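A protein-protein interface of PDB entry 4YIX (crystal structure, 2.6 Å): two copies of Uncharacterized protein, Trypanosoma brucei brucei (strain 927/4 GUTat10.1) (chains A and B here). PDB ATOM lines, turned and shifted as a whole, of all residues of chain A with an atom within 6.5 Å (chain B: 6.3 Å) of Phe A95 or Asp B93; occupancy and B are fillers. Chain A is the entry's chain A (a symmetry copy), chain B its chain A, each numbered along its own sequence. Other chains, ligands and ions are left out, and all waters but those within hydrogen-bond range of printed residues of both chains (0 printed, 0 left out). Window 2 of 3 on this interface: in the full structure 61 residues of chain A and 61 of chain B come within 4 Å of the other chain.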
ATOM      1  N   TYR A  66       0.828   5.697  13.047  1.00  0.00           N
ATOM      2  CA  TYR A  66       1.666   6.194  14.137  1.00  0.00           C
ATOM      3  C   TYR A  66       1.084   7.412  14.862  1.00  0.00           C
ATOM      4  O   TYR A  66       1.314   7.591  16.057  1.00  0.00           O
ATOM      5  CB  TYR A  66       3.070   6.525  13.616  1.00  0.00           C
ATOM      6  CG  TYR A  66       4.109   6.567  14.715  1.00  0.00           C
ATOM      7  CD1 TYR A  66       4.900   5.460  14.993  1.00  0.00           C
ATOM      8  CD2 TYR A  66       4.283   7.710  15.491  1.00  0.00           C
ATOM      9  CE1 TYR A  66       5.841   5.490  16.008  1.00  0.00           C
ATOM     10  CE2 TYR A  66       5.221   7.750  16.510  1.00  0.00           C
ATOM     11  CZ  TYR A  66       5.998   6.639  16.765  1.00  0.00           C
ATOM     12  OH  TYR A  66       6.932   6.679  17.780  1.00  0.00           O
ATOM     13  N   GLN A  91       6.319  11.627  20.389  1.00  0.00           N
ATOM     14  CA  GLN A  91       7.082  11.893  19.202  1.00  0.00           C
ATOM     15  C   GLN A  91       6.182  11.910  17.997  1.00  0.00           C
ATOM     16  O   GLN A  91       5.181  11.272  17.981  1.00  0.00           O
ATOM     17  CB  GLN A  91       8.187  10.836  19.019  1.00  0.00           C
ATOM     18  CG  GLN A  91       8.098   9.619  19.940  1.00  0.00           C
ATOM     19  CD  GLN A  91       9.122   8.566  19.688  1.00  0.00           C
ATOM     20  OE1 GLN A  91       9.267   7.689  20.465  1.00  0.00           O
ATOM     21  NE2 GLN A  91       9.802   8.645  18.599  1.00  0.00           N
ATOM     22  N   ASP A  93       7.349  11.198  14.722  1.00  0.00           N
ATOM     23  CA  ASP A  93       7.729   9.993  13.997  1.00  0.00           C
ATOM     24  C   ASP A  93       8.642   9.143  14.875  1.00  0.00           C
ATOM     25  O   ASP A  93       9.335   9.671  15.747  1.00  0.00           O
ATOM     26  CB  ASP A  93       8.422  10.345  12.680  1.00  0.00           C
ATOM     27  CG  ASP A  93       8.534   9.153  11.739  1.00  0.00           C
ATOM     28  OD1 ASP A  93       7.739   9.073  10.776  1.00  0.00           O
ATOM     29  OD2 ASP A  93       9.414   8.294  11.963  1.00  0.00           O
ATOM     30  N   PRO A  94       8.781   7.920  14.460  1.00  0.00           N
ATOM     31  CA  PRO A  94       9.634   6.954  15.098  1.00  0.00           C
ATOM     32  C   PRO A  94      11.102   7.371  15.070  1.00  0.00           C
ATOM     33  O   PRO A  94      11.799   7.114  16.010  1.00  0.00           O
ATOM     34  CB  PRO A  94       9.356   5.722  14.280  1.00  0.00           C
ATOM     35  CG  PRO A  94       7.915   5.853  14.035  1.00  0.00           C
ATOM     36  CD  PRO A  94       7.577   7.296  13.943  1.00  0.00           C
ATOM     37  N   PHE A  95      11.524   8.006  14.001  1.00  0.00           N
ATOM     38  CA  PHE A  95      12.864   8.507  13.804  1.00  0.00           C
ATOM     39  C   PHE A  95      13.273   9.617  14.769  1.00  0.00           C
ATOM     40  O   PHE A  95      14.425   9.837  15.001  1.00  0.00           O
ATOM     41  CB  PHE A  95      12.925   9.141  12.459  1.00  0.00           C
ATOM     42  CG  PHE A  95      13.215   8.228  11.322  1.00  0.00           C
ATOM     43  CD1 PHE A  95      14.442   8.253  10.732  1.00  0.00           C
ATOM     44  CD2 PHE A  95      12.226   7.484  10.743  1.00  0.00           C
ATOM     45  CE1 PHE A  95      14.701   7.484   9.634  1.00  0.00           C
ATOM     46  CE2 PHE A  95      12.475   6.705   9.649  1.00  0.00           C
ATOM     47  CZ  PHE A  95      13.711   6.714   9.087  1.00  0.00           C
ATOM     48  N   ALA A  96      12.326  10.376  15.258  1.00  0.00           N
ATOM     49  CA  ALA A  96      12.601  11.576  16.011  1.00  0.00           C
ATOM     50  C   ALA A  96      12.931  11.328  17.461  1.00  0.00           C
ATOM     51  O   ALA A  96      13.189  10.216  17.882  1.00  0.00           O
ATOM     52  CB  ALA A  96      11.456  12.542  15.902  1.00  0.00           C
ATOM     53  N   PRO A  97      12.939  12.473  18.254  1.00  0.00           N
ATOM     54  CA  PRO A  97      13.770  12.339  19.443  1.00  0.00           C
ATOM     55  C   PRO A  97      12.579  11.822  20.196  1.00  0.00           C
ATOM     56  O   PRO A  97      11.481  12.142  19.874  1.00  0.00           O
ATOM     57  CB  PRO A  97      13.607  13.675  20.149  1.00  0.00           C
ATOM     58  CG  PRO A  97      13.267  14.627  19.121  1.00  0.00           C
ATOM     59  CD  PRO A  97      12.266  13.856  18.377  1.00  0.00           C
ATOM     60  N   GLY A  98      12.781  10.940  21.117  1.00  0.00           N
ATOM     61  CA  GLY A  98      11.671  10.251  21.695  1.00  0.00           C
ATOM     62  C   GLY A  98      10.694  10.974  22.554  1.00  0.00           C
ATOM     63  O   GLY A  98      10.811  12.103  22.893  1.00  0.00           O
ATOM     64  N   LYS A 193      12.182   6.151  22.815  1.00  0.00           N
ATOM     65  CA  LYS A 193      11.975   6.119  21.380  1.00  0.00           C
ATOM     66  C   LYS A 193      10.958   5.046  21.028  1.00  0.00           C
ATOM     67  O   LYS A 193      11.310   3.877  20.855  1.00  0.00           O
ATOM     68  CB  LYS A 193      13.290   5.869  20.648  1.00  0.00           C
ATOM     69  CG  LYS A 193      14.004   7.132  20.201  1.00  0.00           C
ATOM     70  CD  LYS A 193      14.990   6.830  19.098  1.00  0.00           C
ATOM     71  CE  LYS A 193      15.215   8.036  18.209  1.00  0.00           C
ATOM     72  NZ  LYS A 193      15.826   7.639  16.910  1.00  0.00           N
ATOM     73  N   LEU A 194       9.698   5.458  20.925  1.00  0.00           N
ATOM     74  CA  LEU A 194       8.586   4.560  20.619  1.00  0.00           C
ATOM     75  C   LEU A 194       8.770   3.826  19.303  1.00  0.00           C
ATOM     76  O   LEU A 194       8.860   4.441  18.248  1.00  0.00           O
ATOM     77  CB  LEU A 194       7.278   5.341  20.591  1.00  0.00           C
ATOM     78  CG  LEU A 194       6.836   5.789  21.976  1.00  0.00           C
ATOM     79  CD1 LEU A 194       5.507   6.514  21.903  1.00  0.00           C
ATOM     80  CD2 LEU A 194       6.763   4.579  22.889  1.00  0.00           C
ATOM     81  N   GLY A 196       8.490   1.693  15.859  1.00  0.00           N
ATOM     82  CA  GLY A 196       7.590   1.668  14.726  1.00  0.00           C
ATOM     83  C   GLY A 196       8.346   1.379  13.449  1.00  0.00           C
ATOM     84  O   GLY A 196       8.854   2.295  12.805  1.00  0.00           O
ATOM     85  N   ARG A 199       6.277   2.687   9.325  1.00  0.00           N
ATOM     86  CA  ARG A 199       5.758   3.928   9.816  1.00  0.00           C
ATOM     87  C   ARG A 199       4.499   3.760  10.631  1.00  0.00           C
ATOM     88  O   ARG A 199       3.765   4.699  10.841  1.00  0.00           O
ATOM     89  CB  ARG A 199       5.406   4.766   8.617  1.00  0.00           C
ATOM     90  CG  ARG A 199       4.272   4.155   7.793  1.00  0.00           C
ATOM     91  CD  ARG A 199       4.551   4.125   6.316  1.00  0.00           C
ATOM     92  NE  ARG A 199       4.343   2.822   5.761  1.00  0.00           N
ATOM     93  CZ  ARG A 199       5.164   2.254   4.896  1.00  0.00           C
ATOM     94  NH1 ARG A 199       6.243   2.888   4.512  1.00  0.00           N
ATOM     95  NH2 ARG A 199       4.903   1.059   4.411  1.00  0.00           N
ATOM     96  N   TYR B  66       6.341   6.384  -0.173  1.00  0.00           N
ATOM     97  CA  TYR B  66       7.749   6.763  -0.281  1.00  0.00           C
ATOM     98  C   TYR B  66       8.644   5.665  -0.869  1.00  0.00           C
ATOM     99  O   TYR B  66       9.638   5.963  -1.529  1.00  0.00           O
ATOM    100  CB  TYR B  66       8.289   7.189   1.089  1.00  0.00           C
ATOM    101  CG  TYR B  66       9.537   8.038   0.990  1.00  0.00           C
ATOM    102  CD1 TYR B  66       9.462   9.424   1.025  1.00  0.00           C
ATOM    103  CD2 TYR B  66      10.790   7.452   0.839  1.00  0.00           C
ATOM    104  CE1 TYR B  66      10.600  10.205   0.920  1.00  0.00           C
ATOM    105  CE2 TYR B  66      11.936   8.224   0.731  1.00  0.00           C
ATOM    106  CZ  TYR B  66      11.837   9.600   0.773  1.00  0.00           C
ATOM    107  OH  TYR B  66      12.977  10.369   0.665  1.00  0.00           O
ATOM    108  N   GLN B  91      17.249   6.847  -0.345  1.00  0.00           N
ATOM    109  CA  GLN B  91      17.004   6.783   1.069  1.00  0.00           C
ATOM    110  C   GLN B  91      15.790   5.941   1.349  1.00  0.00           C
ATOM    111  O   GLN B  91      14.919   5.849   0.547  1.00  0.00           O
ATOM    112  CB  GLN B  91      16.812   8.195   1.651  1.00  0.00           C
ATOM    113  CG  GLN B  91      16.661   9.319   0.625  1.00  0.00           C
ATOM    114  CD  GLN B  91      16.386  10.664   1.205  1.00  0.00           C
ATOM    115  OE1 GLN B  91      16.454  11.624   0.521  1.00  0.00           O
ATOM    116  NE2 GLN B  91      16.055  10.723   2.447  1.00  0.00           N
ATOM    117  N   SER B  92      15.803   5.277   2.488  1.00  0.00           N
ATOM    118  CA  SER B  92      14.711   4.500   3.046  1.00  0.00           C
ATOM    119  C   SER B  92      13.516   5.265   3.591  1.00  0.00           C
ATOM    120  O   SER B  92      12.381   4.871   3.475  1.00  0.00           O
ATOM    121  CB  SER B  92      15.270   3.619   4.135  1.00  0.00           C
ATOM    122  OG  SER B  92      15.300   4.291   5.372  1.00  0.00           O
ATOM    123  N   ASP B  93      13.814   6.338   4.270  1.00  0.00           N
ATOM    124  CA  ASP B  93      12.828   7.307   4.731  1.00  0.00           C
ATOM    125  C   ASP B  93      13.353   8.717   4.482  1.00  0.00           C
ATOM    126  O   ASP B  93      14.566   8.933   4.444  1.00  0.00           O
ATOM    127  CB  ASP B  93      12.514   7.103   6.214  1.00  0.00           C
ATOM    128  CG  ASP B  93      11.264   7.851   6.656  1.00  0.00           C
ATOM    129  OD1 ASP B  93      10.202   7.207   6.808  1.00  0.00           O
ATOM    130  OD2 ASP B  93      11.342   9.083   6.852  1.00  0.00           O
ATOM    131  N   PRO B  94      12.440   9.640   4.559  1.00  0.00           N
ATOM    132  CA  PRO B  94      12.712  11.044   4.412  1.00  0.00           C
ATOM    133  C   PRO B  94      13.654  11.565   5.494  1.00  0.00           C
ATOM    134  O   PRO B  94      14.458  12.408   5.210  1.00  0.00           O
ATOM    135  CB  PRO B  94      11.329  11.627   4.503  1.00  0.00           C
ATOM    136  CG  PRO B  94      10.540  10.628   3.774  1.00  0.00           C
ATOM    137  CD  PRO B  94      11.153   9.291   3.986  1.00  0.00           C
ATOM    138  N   PHE B  95      13.533  11.048   6.694  1.00  0.00           N
ATOM    139  CA  PHE B  95      14.351  11.388   7.835  1.00  0.00           C
ATOM    140  C   PHE B  95      15.823  11.012   7.693  1.00  0.00           C
ATOM    141  O   PHE B  95      16.665  11.571   8.333  1.00  0.00           O
ATOM    142  CB  PHE B  95      13.872  10.592   8.998  1.00  0.00           C
ATOM    143  CG  PHE B  95      12.745  11.178   9.768  1.00  0.00           C
ATOM    144  CD1 PHE B  95      12.974  11.721  10.996  1.00  0.00           C
ATOM    145  CD2 PHE B  95      11.452  11.033   9.350  1.00  0.00           C
ATOM    146  CE1 PHE B  95      11.940  12.188  11.754  1.00  0.00           C
ATOM    147  CE2 PHE B  95      10.410  11.502  10.096  1.00  0.00           C
ATOM    148  CZ  PHE B  95      10.653  12.070  11.305  1.00  0.00           C
ATOM    149  N   ALA B  96      16.119  10.000   6.919  1.00  0.00           N
ATOM    150  CA  ALA B  96      17.440   9.422   6.865  1.00  0.00           C
ATOM    151  C   ALA B  96      18.402  10.174   5.980  1.00  0.00           C
ATOM    152  O   ALA B  96      18.156  11.291   5.564  1.00  0.00           O
ATOM    153  CB  ALA B  96      17.370   7.982   6.442  1.00  0.00           C
ATOM    154  N   PRO B  97      19.587   9.493   5.708  1.00  0.00           N
ATOM    155  CA  PRO B  97      20.689  10.381   5.364  1.00  0.00           C
ATOM    156  C   PRO B  97      20.298  10.281   3.919  1.00  0.00           C
ATOM    157  O   PRO B  97      19.737   9.314   3.515  1.00  0.00           O
ATOM    158  CB  PRO B  97      21.845   9.433   5.093  1.00  0.00           C
ATOM    159  CG  PRO B  97      21.562   8.238   5.848  1.00  0.00           C
ATOM    160  CD  PRO B  97      20.141   8.065   5.533  1.00  0.00           C
ATOM    161  N   LEU B 194      15.669  13.717  -0.094  1.00  0.00           N
ATOM    162  CA  LEU B 194      14.405  13.689  -0.827  1.00  0.00           C
ATOM    163  C   LEU B 194      13.211  14.029   0.048  1.00  0.00           C
ATOM    164  O   LEU B 194      12.926  13.338   1.017  1.00  0.00           O
ATOM    165  CB  LEU B 194      14.201  12.318  -1.460  1.00  0.00           C
ATOM    166  CG  LEU B 194      15.146  12.066  -2.625  1.00  0.00           C
ATOM    167  CD1 LEU B 194      14.870  10.716  -3.254  1.00  0.00           C
ATOM    168  CD2 LEU B 194      15.002  13.192  -3.633  1.00  0.00           C
ATOM    169  N   GLY B 196       9.593  14.644   1.788  1.00  0.00           N
ATOM    170  CA  GLY B 196       8.401  13.852   2.006  1.00  0.00           C
ATOM    171  C   GLY B 196       7.772  14.190   3.338  1.00  0.00           C
ATOM    172  O   GLY B 196       8.133  13.613   4.361  1.00  0.00           O
ATOM    173  N   ARG B 199       4.835  10.930   5.273  1.00  0.00           N
ATOM    174  CA  ARG B 199       5.622   9.793   4.899  1.00  0.00           C
ATOM    175  C   ARG B 199       5.440   9.399   3.453  1.00  0.00           C
ATOM    176  O   ARG B 199       5.761   8.301   3.064  1.00  0.00           O
ATOM    177  CB  ARG B 199       5.156   8.636   5.740  1.00  0.00           C
ATOM    178  CG  ARG B 199       3.709   8.243   5.436  1.00  0.00           C
ATOM    179  CD  ARG B 199       2.867   8.052   6.666  1.00  0.00           C
ATOM    180  NE  ARG B 199       1.647   8.799   6.597  1.00  0.00           N
ATOM    181  CZ  ARG B 199       1.156   9.495   7.606  1.00  0.00           C
ATOM    182  NH1 ARG B 199       1.801   9.533   8.745  1.00  0.00           N
ATOM    183  NH2 ARG B 199       0.019  10.145   7.480  1.00  0.00           N
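The backbone carbonyl oxygen of Asp B93 is in hydrogen-bond range of the side-chain amide nitrogen of Gln B91, 3.1 Å away. The side-chain carboxylate of Asp B93 lies within hydrogen-bond range of the backbone NH of Phe B95, at 2.9 Å. NE2 of Gln A91 is in hydrogen-bond range of O of Asp A93, 3.1 Å away. OD2 of Asp A93 sits at hydrogen-bond distance from N of Phe A95 (2.9 Å). The backbone carbonyl oxygen of Phe A95 is in hydrogen-bond range of the side-chain amino group of Lys A193.
Among the printed residues, pairs that only touch across the chains: Asp A93 with Phe B95 (3.1 Å), Phe A95 with Asp B93 (3.1 Å), Phe A95 with Phe B95 (3.0 Å), Phe A95 with Ala B96 (3.96 Å) and Ala A96 with Phe B95 (3.96 Å).
Of the printed residues of chain B, Asp A93 touches Phe B95 (3.1 Å). Of chain B, only Asp B93 (3.1 Å), Phe B95 (3.0 Å) and Ala B96 (3.96 Å) come within 4 Å of Phe A95. Printed residues of chain B within 4 Å of Ala A96: Phe B95. Asp B93 touches one residue of chain A. Of the printed residues of chain A, Phe B95 touches Asp A93 (3.1 Å), Phe A95 (3.0 Å) and Ala A96 (3.96 Å). The nearest residue of chain A that does not touch Asp B93 is Asp A93 (5.0 Å). The nearest printed residue of chain A that does not touch Ala B96 is Asp A93 (8.6 Å).
Printed residues of chain A that touch a printed residue of chain B: Asp A93, Phe A95 and Ala A96. Hydrophobic or aromatic side chains of chain A within 4 Å of the printed part of chain B: Phe A95. Hydrophobic or aromatic side chains of chain B that line the printed part of chain A: Phe B95.
Asp A93 touches Phe B95, and with the chains exchanged Phe A95 touches Asp B93. Phe A95 touches its own counterpart, Phe B95. Phe A95 touches Ala B96, and with the chains exchanged Ala A96 touches Phe B95. Positions printed for both chains: 66, 91, 93, 94, 95, 96, 97, 194, 196 and 199. Of the 5 pairs that touch across the chains among the printed residues, 5 have their exchanged pair printed and touching as well.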
